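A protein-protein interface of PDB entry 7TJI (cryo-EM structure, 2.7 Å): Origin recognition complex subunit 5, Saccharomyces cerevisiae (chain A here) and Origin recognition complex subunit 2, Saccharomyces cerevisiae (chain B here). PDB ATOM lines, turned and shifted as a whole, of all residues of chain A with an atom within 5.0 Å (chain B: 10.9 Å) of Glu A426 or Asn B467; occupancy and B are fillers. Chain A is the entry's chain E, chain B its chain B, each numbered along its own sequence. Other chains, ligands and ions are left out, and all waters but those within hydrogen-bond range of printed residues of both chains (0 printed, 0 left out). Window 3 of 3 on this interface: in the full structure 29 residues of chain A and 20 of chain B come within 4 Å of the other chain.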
ATOM      1  N   PHE A 421      28.475   2.940  10.104  1.00  0.00           N
ATOM      2  CA  PHE A 421      29.082   3.562  11.276  1.00  0.00           C
ATOM      3  C   PHE A 421      28.535   2.977  12.569  1.00  0.00           C
ATOM      4  O   PHE A 421      29.278   2.854  13.551  1.00  0.00           O
ATOM      5  CB  PHE A 421      28.876   5.071  11.224  1.00  0.00           C
ATOM      6  CG  PHE A 421      29.840   5.768  10.317  1.00  0.00           C
ATOM      7  CD1 PHE A 421      29.552   5.931   8.972  1.00  0.00           C
ATOM      8  CD2 PHE A 421      31.050   6.235  10.802  1.00  0.00           C
ATOM      9  CE1 PHE A 421      30.446   6.565   8.131  1.00  0.00           C
ATOM     10  CE2 PHE A 421      31.948   6.867   9.966  1.00  0.00           C
ATOM     11  CZ  PHE A 421      31.645   7.033   8.629  1.00  0.00           C
ATOM     12  N   GLN A 422      27.258   2.586  12.574  1.00  0.00           N
ATOM     13  CA  GLN A 422      26.685   1.906  13.731  1.00  0.00           C
ATOM     14  C   GLN A 422      27.343   0.549  13.954  1.00  0.00           C
ATOM     15  O   GLN A 422      27.632   0.171  15.096  1.00  0.00           O
ATOM     16  CB  GLN A 422      25.176   1.755  13.548  1.00  0.00           C
ATOM     17  CG  GLN A 422      24.414   1.503  14.830  1.00  0.00           C
ATOM     18  CD  GLN A 422      22.936   1.271  14.591  1.00  0.00           C
ATOM     19  OE1 GLN A 422      22.321   1.920  13.747  1.00  0.00           O
ATOM     20  NE2 GLN A 422      22.357   0.343  15.338  1.00  0.00           N
ATOM     21  N   ASN A 423      27.616  -0.180  12.866  1.00  0.00           N
ATOM     22  CA  ASN A 423      28.293  -1.469  12.966  1.00  0.00           C
ATOM     23  C   ASN A 423      29.734  -1.315  13.436  1.00  0.00           C
ATOM     24  O   ASN A 423      30.218  -2.130  14.229  1.00  0.00           O
ATOM     25  CB  ASN A 423      28.237  -2.183  11.620  1.00  0.00           C
ATOM     26  CG  ASN A 423      26.909  -2.861  11.387  1.00  0.00           C
ATOM     27  OD1 ASN A 423      26.462  -3.663  12.202  1.00  0.00           O
ATOM     28  ND2 ASN A 423      26.264  -2.533  10.279  1.00  0.00           N
ATOM     29  N   LEU A 424      30.430  -0.284  12.953  1.00  0.00           N
ATOM     30  CA  LEU A 424      31.799  -0.022  13.390  1.00  0.00           C
ATOM     31  C   LEU A 424      31.851   0.364  14.867  1.00  0.00           C
ATOM     32  O   LEU A 424      32.751  -0.072  15.602  1.00  0.00           O
ATOM     33  CB  LEU A 424      32.404   1.070  12.513  1.00  0.00           C
ATOM     34  CG  LEU A 424      33.885   1.441  12.589  1.00  0.00           C
ATOM     35  CD1 LEU A 424      34.786   0.227  12.727  1.00  0.00           C
ATOM     36  CD2 LEU A 424      34.243   2.237  11.356  1.00  0.00           C
ATOM     37  N   SER A 425      30.879   1.168  15.318  1.00  0.00           N
ATOM     38  CA  SER A 425      30.769   1.511  16.733  1.00  0.00           C
ATOM     39  C   SER A 425      30.487   0.278  17.583  1.00  0.00           C
ATOM     40  O   SER A 425      31.023   0.142  18.692  1.00  0.00           O
ATOM     41  CB  SER A 425      29.669   2.557  16.921  1.00  0.00           C
ATOM     42  OG  SER A 425      29.938   3.404  18.021  1.00  0.00           O
ATOM     43  N   GLU A 426      29.645  -0.628  17.077  1.00  0.00           N
ATOM     44  CA  GLU A 426      29.385  -1.876  17.785  1.00  0.00           C
ATOM     45  C   GLU A 426      30.633  -2.746  17.858  1.00  0.00           C
ATOM     46  O   GLU A 426      30.901  -3.361  18.896  1.00  0.00           O
ATOM     47  CB  GLU A 426      28.241  -2.635  17.114  1.00  0.00           C
ATOM     48  CG  GLU A 426      27.659  -3.755  17.960  1.00  0.00           C
ATOM     49  CD  GLU A 426      27.324  -3.327  19.377  1.00  0.00           C
ATOM     50  OE1 GLU A 426      26.650  -2.288  19.552  1.00  0.00           O
ATOM     51  OE2 GLU A 426      27.735  -4.033  20.322  1.00  0.00           O
ATOM     52  N   LEU A 427      31.414  -2.791  16.771  1.00  0.00           N
ATOM     53  CA  LEU A 427      32.671  -3.537  16.759  1.00  0.00           C
ATOM     54  C   LEU A 427      33.653  -2.986  17.783  1.00  0.00           C
ATOM     55  O   LEU A 427      34.389  -3.748  18.418  1.00  0.00           O
ATOM     56  CB  LEU A 427      33.295  -3.504  15.361  1.00  0.00           C
ATOM     57  CG  LEU A 427      32.711  -4.431  14.295  1.00  0.00           C
ATOM     58  CD1 LEU A 427      33.347  -4.168  12.947  1.00  0.00           C
ATOM     59  CD2 LEU A 427      32.895  -5.882  14.692  1.00  0.00           C
ATOM     60  N   HIS A 428      33.672  -1.662  17.961  1.00  0.00           N
ATOM     61  CA  HIS A 428      34.451  -1.098  19.059  1.00  0.00           C
ATOM     62  C   HIS A 428      33.869  -1.469  20.421  1.00  0.00           C
ATOM     63  O   HIS A 428      34.624  -1.640  21.384  1.00  0.00           O
ATOM     64  CB  HIS A 428      34.558   0.418  18.927  1.00  0.00           C
ATOM     65  CG  HIS A 428      35.471   1.042  19.937  1.00  0.00           C
ATOM     66  ND1 HIS A 428      35.034   1.475  21.169  1.00  0.00           N
ATOM     67  CD2 HIS A 428      36.802   1.279  19.908  1.00  0.00           C
ATOM     68  CE1 HIS A 428      36.054   1.966  21.849  1.00  0.00           C
ATOM     69  NE2 HIS A 428      37.139   1.859  21.106  1.00  0.00           N
ATOM     70  N   THR A 429      32.542  -1.592  20.524  1.00  0.00           N
ATOM     71  CA  THR A 429      31.936  -2.013  21.787  1.00  0.00           C
ATOM     72  C   THR A 429      32.256  -3.476  22.102  1.00  0.00           C
ATOM     73  O   THR A 429      32.595  -3.808  23.245  1.00  0.00           O
ATOM     74  CB  THR A 429      30.423  -1.759  21.747  1.00  0.00           C
ATOM     75  OG1 THR A 429      30.177  -0.350  21.791  1.00  0.00           O
ATOM     76  CG2 THR A 429      29.698  -2.421  22.918  1.00  0.00           C
ATOM     77  N   LEU A 430      32.222  -4.358  21.097  1.00  0.00           N
ATOM     78  CA  LEU A 430      32.519  -5.773  21.319  1.00  0.00           C
ATOM     79  C   LEU A 430      34.007  -6.076  21.491  1.00  0.00           C
ATOM     80  O   LEU A 430      34.361  -7.258  21.568  1.00  0.00           O
ATOM     81  CB  LEU A 430      31.996  -6.650  20.174  1.00  0.00           C
ATOM     82  CG  LEU A 430      30.550  -6.673  19.671  1.00  0.00           C
ATOM     83  CD1 LEU A 430      30.495  -6.465  18.170  1.00  0.00           C
ATOM     84  CD2 LEU A 430      29.877  -7.970  20.047  1.00  0.00           C
ATOM     85  N   ASN B 435      31.800   9.735  26.033  1.00  0.00           N
ATOM     86  CA  ASN B 435      30.942   8.563  26.183  1.00  0.00           C
ATOM     87  C   ASN B 435      29.934   8.726  27.317  1.00  0.00           C
ATOM     88  O   ASN B 435      28.794   8.261  27.204  1.00  0.00           O
ATOM     89  CB  ASN B 435      31.806   7.320  26.405  1.00  0.00           C
ATOM     90  CG  ASN B 435      31.001   6.047  26.385  1.00  0.00           C
ATOM     91  OD1 ASN B 435      30.598   5.572  25.326  1.00  0.00           O
ATOM     92  ND2 ASN B 435      30.750   5.488  27.562  1.00  0.00           N
ATOM     93  N   SER B 442      21.361   9.503  25.801  1.00  0.00           N
ATOM     94  CA  SER B 442      20.560   8.428  25.218  1.00  0.00           C
ATOM     95  C   SER B 442      19.605   7.824  26.244  1.00  0.00           C
ATOM     96  O   SER B 442      18.443   7.534  25.918  1.00  0.00           O
ATOM     97  CB  SER B 442      21.463   7.358  24.604  1.00  0.00           C
ATOM     98  OG  SER B 442      22.752   7.377  25.178  1.00  0.00           O
ATOM     99  N   PHE B 443      20.057   7.657  27.499  1.00  0.00           N
ATOM    100  CA  PHE B 443      19.119   7.245  28.543  1.00  0.00           C
ATOM    101  C   PHE B 443      18.069   8.312  28.840  1.00  0.00           C
ATOM    102  O   PHE B 443      16.953   7.973  29.243  1.00  0.00           O
ATOM    103  CB  PHE B 443      19.845   6.858  29.831  1.00  0.00           C
ATOM    104  CG  PHE B 443      20.601   5.570  29.744  1.00  0.00           C
ATOM    105  CD1 PHE B 443      20.056   4.486  29.077  1.00  0.00           C
ATOM    106  CD2 PHE B 443      21.814   5.412  30.392  1.00  0.00           C
ATOM    107  CE1 PHE B 443      20.731   3.284  29.011  1.00  0.00           C
ATOM    108  CE2 PHE B 443      22.489   4.206  30.339  1.00  0.00           C
ATOM    109  CZ  PHE B 443      21.951   3.145  29.643  1.00  0.00           C
ATOM    110  N   VAL B 446      15.432   7.809  26.216  1.00  0.00           N
ATOM    111  CA  VAL B 446      14.530   6.683  26.473  1.00  0.00           C
ATOM    112  C   VAL B 446      13.177   7.176  26.996  1.00  0.00           C
ATOM    113  O   VAL B 446      12.120   6.652  26.620  1.00  0.00           O
ATOM    114  CB  VAL B 446      15.200   5.692  27.447  1.00  0.00           C
ATOM    115  CG1 VAL B 446      14.243   4.606  27.908  1.00  0.00           C
ATOM    116  CG2 VAL B 446      16.423   5.064  26.801  1.00  0.00           C
ATOM    117  N   PRO B 462      27.870   9.769  13.103  1.00  0.00           N
ATOM    118  CA  PRO B 462      27.224   8.472  13.396  1.00  0.00           C
ATOM    119  C   PRO B 462      28.140   7.388  13.958  1.00  0.00           C
ATOM    120  O   PRO B 462      27.625   6.363  14.420  1.00  0.00           O
ATOM    121  CB  PRO B 462      26.665   8.047  12.038  1.00  0.00           C
ATOM    122  CG  PRO B 462      26.465   9.287  11.335  1.00  0.00           C
ATOM    123  CD  PRO B 462      27.582  10.145  11.700  1.00  0.00           C
ATOM    124  N   LEU B 463      29.462   7.584  13.951  1.00  0.00           N
ATOM    125  CA  LEU B 463      30.377   6.687  14.645  1.00  0.00           C
ATOM    126  C   LEU B 463      30.198   6.713  16.160  1.00  0.00           C
ATOM    127  O   LEU B 463      30.646   5.781  16.836  1.00  0.00           O
ATOM    128  CB  LEU B 463      31.818   7.051  14.283  1.00  0.00           C
ATOM    129  CG  LEU B 463      32.956   6.064  14.520  1.00  0.00           C
ATOM    130  CD1 LEU B 463      32.720   4.807  13.724  1.00  0.00           C
ATOM    131  CD2 LEU B 463      34.275   6.704  14.151  1.00  0.00           C
ATOM    132  N   LEU B 464      29.549   7.746  16.712  1.00  0.00           N
ATOM    133  CA  LEU B 464      29.370   7.820  18.159  1.00  0.00           C
ATOM    134  C   LEU B 464      28.398   6.777  18.702  1.00  0.00           C
ATOM    135  O   LEU B 464      28.466   6.450  19.890  1.00  0.00           O
ATOM    136  CB  LEU B 464      28.888   9.215  18.557  1.00  0.00           C
ATOM    137  CG  LEU B 464      29.886  10.367  18.423  1.00  0.00           C
ATOM    138  CD1 LEU B 464      29.220  11.686  18.759  1.00  0.00           C
ATOM    139  CD2 LEU B 464      31.099  10.127  19.309  1.00  0.00           C
ATOM    140  N   TRP B 465      27.513   6.235  17.872  1.00  0.00           N
ATOM    141  CA  TRP B 465      26.353   5.492  18.349  1.00  0.00           C
ATOM    142  C   TRP B 465      26.453   4.024  17.960  1.00  0.00           C
ATOM    143  O   TRP B 465      26.396   3.683  16.774  1.00  0.00           O
ATOM    144  CB  TRP B 465      25.070   6.118  17.804  1.00  0.00           C
ATOM    145  CG  TRP B 465      25.060   7.604  17.987  1.00  0.00           C
ATOM    146  CD1 TRP B 465      25.372   8.289  19.125  1.00  0.00           C
ATOM    147  CD2 TRP B 465      24.757   8.589  16.998  1.00  0.00           C
ATOM    148  NE1 TRP B 465      25.272   9.637  18.908  1.00  0.00           N
ATOM    149  CE2 TRP B 465      24.894   9.849  17.610  1.00  0.00           C
ATOM    150  CE3 TRP B 465      24.375   8.529  15.655  1.00  0.00           C
ATOM    151  CZ2 TRP B 465      24.664  11.036  16.925  1.00  0.00           C
ATOM    152  CZ3 TRP B 465      24.148   9.707  14.979  1.00  0.00           C
ATOM    153  CH2 TRP B 465      24.294  10.945  15.614  1.00  0.00           C
ATOM    154  N   ASP B 466      26.584   3.159  18.964  1.00  0.00           N
ATOM    155  CA  ASP B 466      26.477   1.721  18.766  1.00  0.00           C
ATOM    156  C   ASP B 466      24.998   1.326  18.817  1.00  0.00           C
ATOM    157  O   ASP B 466      24.110   2.180  18.801  1.00  0.00           O
ATOM    158  CB  ASP B 466      27.344   0.975  19.780  1.00  0.00           C
ATOM    159  CG  ASP B 466      26.971   1.269  21.231  1.00  0.00           C
ATOM    160  OD1 ASP B 466      26.183   2.201  21.497  1.00  0.00           O
ATOM    161  OD2 ASP B 466      27.478   0.553  22.118  1.00  0.00           O
ATOM    162  N   ASN B 467      24.718   0.025  18.890  1.00  0.00           N
ATOM    163  CA  ASN B 467      23.348  -0.451  18.719  1.00  0.00           C
ATOM    164  C   ASN B 467      22.472  -0.117  19.922  1.00  0.00           C
ATOM    165  O   ASN B 467      21.291   0.217  19.760  1.00  0.00           O
ATOM    166  CB  ASN B 467      23.361  -1.952  18.443  1.00  0.00           C
ATOM    167  CG  ASN B 467      23.826  -2.274  17.040  1.00  0.00           C
ATOM    168  OD1 ASN B 467      24.767  -1.666  16.535  1.00  0.00           O
ATOM    169  ND2 ASN B 467      23.170  -3.230  16.402  1.00  0.00           N
ATOM    170  N   MET B 468      23.041  -0.172  21.129  1.00  0.00           N
ATOM    171  CA  MET B 468      22.315   0.235  22.329  1.00  0.00           C
ATOM    172  C   MET B 468      21.993   1.726  22.309  1.00  0.00           C
ATOM    173  O   MET B 468      20.857   2.128  22.592  1.00  0.00           O
ATOM    174  CB  MET B 468      23.132  -0.121  23.572  1.00  0.00           C
ATOM    175  CG  MET B 468      22.361  -0.145  24.885  1.00  0.00           C
ATOM    176  SD  MET B 468      21.265  -1.563  25.107  1.00  0.00           S
ATOM    177  CE  MET B 468      19.673  -0.853  24.709  1.00  0.00           C
ATOM    178  N   LYS B 469      22.970   2.558  21.942  1.00  0.00           N
ATOM    179  CA  LYS B 469      22.739   3.997  21.916  1.00  0.00           C
ATOM    180  C   LYS B 469      21.851   4.412  20.750  1.00  0.00           C
ATOM    181  O   LYS B 469      21.066   5.354  20.886  1.00  0.00           O
ATOM    182  CB  LYS B 469      24.069   4.745  21.872  1.00  0.00           C
ATOM    183  CG  LYS B 469      24.723   4.894  23.235  1.00  0.00           C
ATOM    184  CD  LYS B 469      25.934   5.801  23.172  1.00  0.00           C
ATOM    185  CE  LYS B 469      26.802   5.641  24.404  1.00  0.00           C
ATOM    186  NZ  LYS B 469      28.136   5.087  24.067  1.00  0.00           N
ATOM    187  N   ALA B 470      21.949   3.725  19.607  1.00  0.00           N
ATOM    188  CA  ALA B 470      21.057   4.036  18.495  1.00  0.00           C
ATOM    189  C   ALA B 470      19.632   3.589  18.779  1.00  0.00           C
ATOM    190  O   ALA B 470      18.684   4.215  18.295  1.00  0.00           O
ATOM    191  CB  ALA B 470      21.553   3.398  17.199  1.00  0.00           C
ATOM    192  N   GLN B 471      19.460   2.508  19.542  1.00  0.00           N
ATOM    193  CA  GLN B 471      18.120   2.126  19.972  1.00  0.00           C
ATOM    194  C   GLN B 471      17.555   3.125  20.973  1.00  0.00           C
ATOM    195  O   GLN B 471      16.384   3.509  20.878  1.00  0.00           O
ATOM    196  CB  GLN B 471      18.137   0.724  20.574  1.00  0.00           C
ATOM    197  CG  GLN B 471      16.766   0.260  20.994  1.00  0.00           C
ATOM    198  CD  GLN B 471      16.755  -1.130  21.559  1.00  0.00           C
ATOM    199  OE1 GLN B 471      16.645  -2.107  20.823  1.00  0.00           O
ATOM    200  NE2 GLN B 471      16.845  -1.232  22.874  1.00  0.00           N
ATOM    201  N   ASN B 472      18.377   3.565  21.928  1.00  0.00           N
ATOM    202  CA  ASN B 472      17.912   4.488  22.957  1.00  0.00           C
ATOM    203  C   ASN B 472      17.613   5.869  22.396  1.00  0.00           C
ATOM    204  O   ASN B 472      16.691   6.541  22.869  1.00  0.00           O
ATOM    205  CB  ASN B 472      18.951   4.590  24.068  1.00  0.00           C
ATOM    206  CG  ASN B 472      18.978   3.369  24.944  1.00  0.00           C
ATOM    207  OD1 ASN B 472      18.113   2.502  24.843  1.00  0.00           O
ATOM    208  ND2 ASN B 472      19.975   3.287  25.811  1.00  0.00           N
ATOM    209  N   TYR B 473      18.385   6.312  21.404  1.00  0.00           N
ATOM    210  CA  TYR B 473      18.161   7.628  20.823  1.00  0.00           C
ATOM    211  C   TYR B 473      16.886   7.664  19.991  1.00  0.00           C
ATOM    212  O   TYR B 473      16.124   8.631  20.083  1.00  0.00           O
ATOM    213  CB  TYR B 473      19.366   8.040  19.984  1.00  0.00           C
ATOM    214  CG  TYR B 473      20.394   8.842  20.742  1.00  0.00           C
ATOM    215  CD1 TYR B 473      20.013   9.897  21.560  1.00  0.00           C
ATOM    216  CD2 TYR B 473      21.747   8.551  20.629  1.00  0.00           C
ATOM    217  CE1 TYR B 473      20.955  10.639  22.250  1.00  0.00           C
ATOM    218  CE2 TYR B 473      22.691   9.282  21.314  1.00  0.00           C
ATOM    219  CZ  TYR B 473      22.291  10.324  22.122  1.00  0.00           C
ATOM    220  OH  TYR B 473      23.232  11.056  22.801  1.00  0.00           O
ATOM    221  N   ASN B 474      16.637   6.614  19.197  1.00  0.00           N
ATOM    222  CA  ASN B 474      15.466   6.476  18.316  1.00  0.00           C
ATOM    223  C   ASN B 474      15.363   7.654  17.338  1.00  0.00           C
ATOM    224  O   ASN B 474      14.385   8.399  17.308  1.00  0.00           O
ATOM    225  CB  ASN B 474      14.179   6.299  19.138  1.00  0.00           C
ATOM    226  CG  ASN B 474      13.015   5.786  18.317  1.00  0.00           C
ATOM    227  OD1 ASN B 474      11.903   6.297  18.423  1.00  0.00           O
ATOM    228  ND2 ASN B 474      13.260   4.772  17.504  1.00  0.00           N
ATOM    229  N   PHE B 475      16.412   7.802  16.535  1.00  0.00           N
ATOM    230  CA  PHE B 475      16.594   8.990  15.714  1.00  0.00           C
ATOM    231  C   PHE B 475      15.806   8.901  14.413  1.00  0.00           C
ATOM    232  O   PHE B 475      15.860   7.888  13.710  1.00  0.00           O
ATOM    233  CB  PHE B 475      18.076   9.184  15.393  1.00  0.00           C
ATOM    234  CG  PHE B 475      18.840   9.934  16.441  1.00  0.00           C
ATOM    235  CD1 PHE B 475      18.246  10.959  17.159  1.00  0.00           C
ATOM    236  CD2 PHE B 475      20.171   9.629  16.688  1.00  0.00           C
ATOM    237  CE1 PHE B 475      18.959  11.656  18.115  1.00  0.00           C
ATOM    238  CE2 PHE B 475      20.891  10.323  17.641  1.00  0.00           C
ATOM    239  CZ  PHE B 475      20.280  11.336  18.357  1.00  0.00           C
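Phe A421 touches Pro B462.
CD2 of Phe A421 touches CD1 of Leu B463 (3.7 Å).
Gln A422 touches Trp B465.
CD of Gln A422 touches CB of Ala B470, 3.6 Å away.
Leu A424 touches Leu B463.
Ser A425 touches Leu B464 (OG to C, 3.8 Å).
O of Trp B465 touches CB of Ser A425, 3.5 Å away.
Glu A426 touches Asp B466 (OE1 to CB, 3.3 Å).
OD1 of Asn B467 sits at hydrogen-bond distance from NE2 of Gln A422.
The side-chain hydroxyl of Thr A429 sits at hydrogen-bond distance from the side-chain carboxylate of Asp B466 (2.9 Å).
N of Asp B466 sits at hydrogen-bond distance from OG of Ser A425 (3.5 Å).
The backbone NH of Asn B467 lies within hydrogen-bond range of the side-chain carboxylate of Glu A426 (3.1 Å).
The backbone carbonyl oxygen of Leu B463 lies within hydrogen-bond range of the side-chain hydroxyl of Ser A425 (2.7 Å).
Glu A426 touches just these residues of chain B: Asp B466 and Asn B467.
Of chain A, only Gln A422 (3.4 Å) and Glu A426 (3.1 Å) come within 4 Å of Asn B467.
No residue of chain B comes within 4 Å of Asn A423.
No residue of chain B comes within 4 Å of Leu A427.
Printed residues of chain A within 4 Å of Ala B470: Gln A422.
Printed residues of chain A within 4 Å of Leu B463: Phe A421 (3.7 Å), Leu A424 (3.7 Å) and Ser A425 (2.7 Å).
Of the printed residues of chain A, Asp B466 touches Ser A425 (3.5 Å), Glu A426 (3.3 Å) and Thr A429 (2.9 Å).
The nearest residue of chain B that does not touch Glu A426 is Met B468 (4.5 Å).
The nearest residue of chain A that does not touch Asn B467 is Asn A423 (4.9 Å).
Of the 10 printed residues of chain A, 6 touch a printed residue of chain B.
Hydrophobic or aromatic side chains of chain A within 4 Å of the printed part of chain B: Phe A421 and Leu A424.
Of the 18 printed residues of chain B, 7 touch a printed residue of chain A.
Among the printed residues, 13 pairs touch across the chains.
O of Ser A425 sits at hydrogen-bond distance from OG1 of Thr A429 (3.2 Å).
OD1 of Asp B466 is in hydrogen-bond range of N of Lys B469 (3.3 Å).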
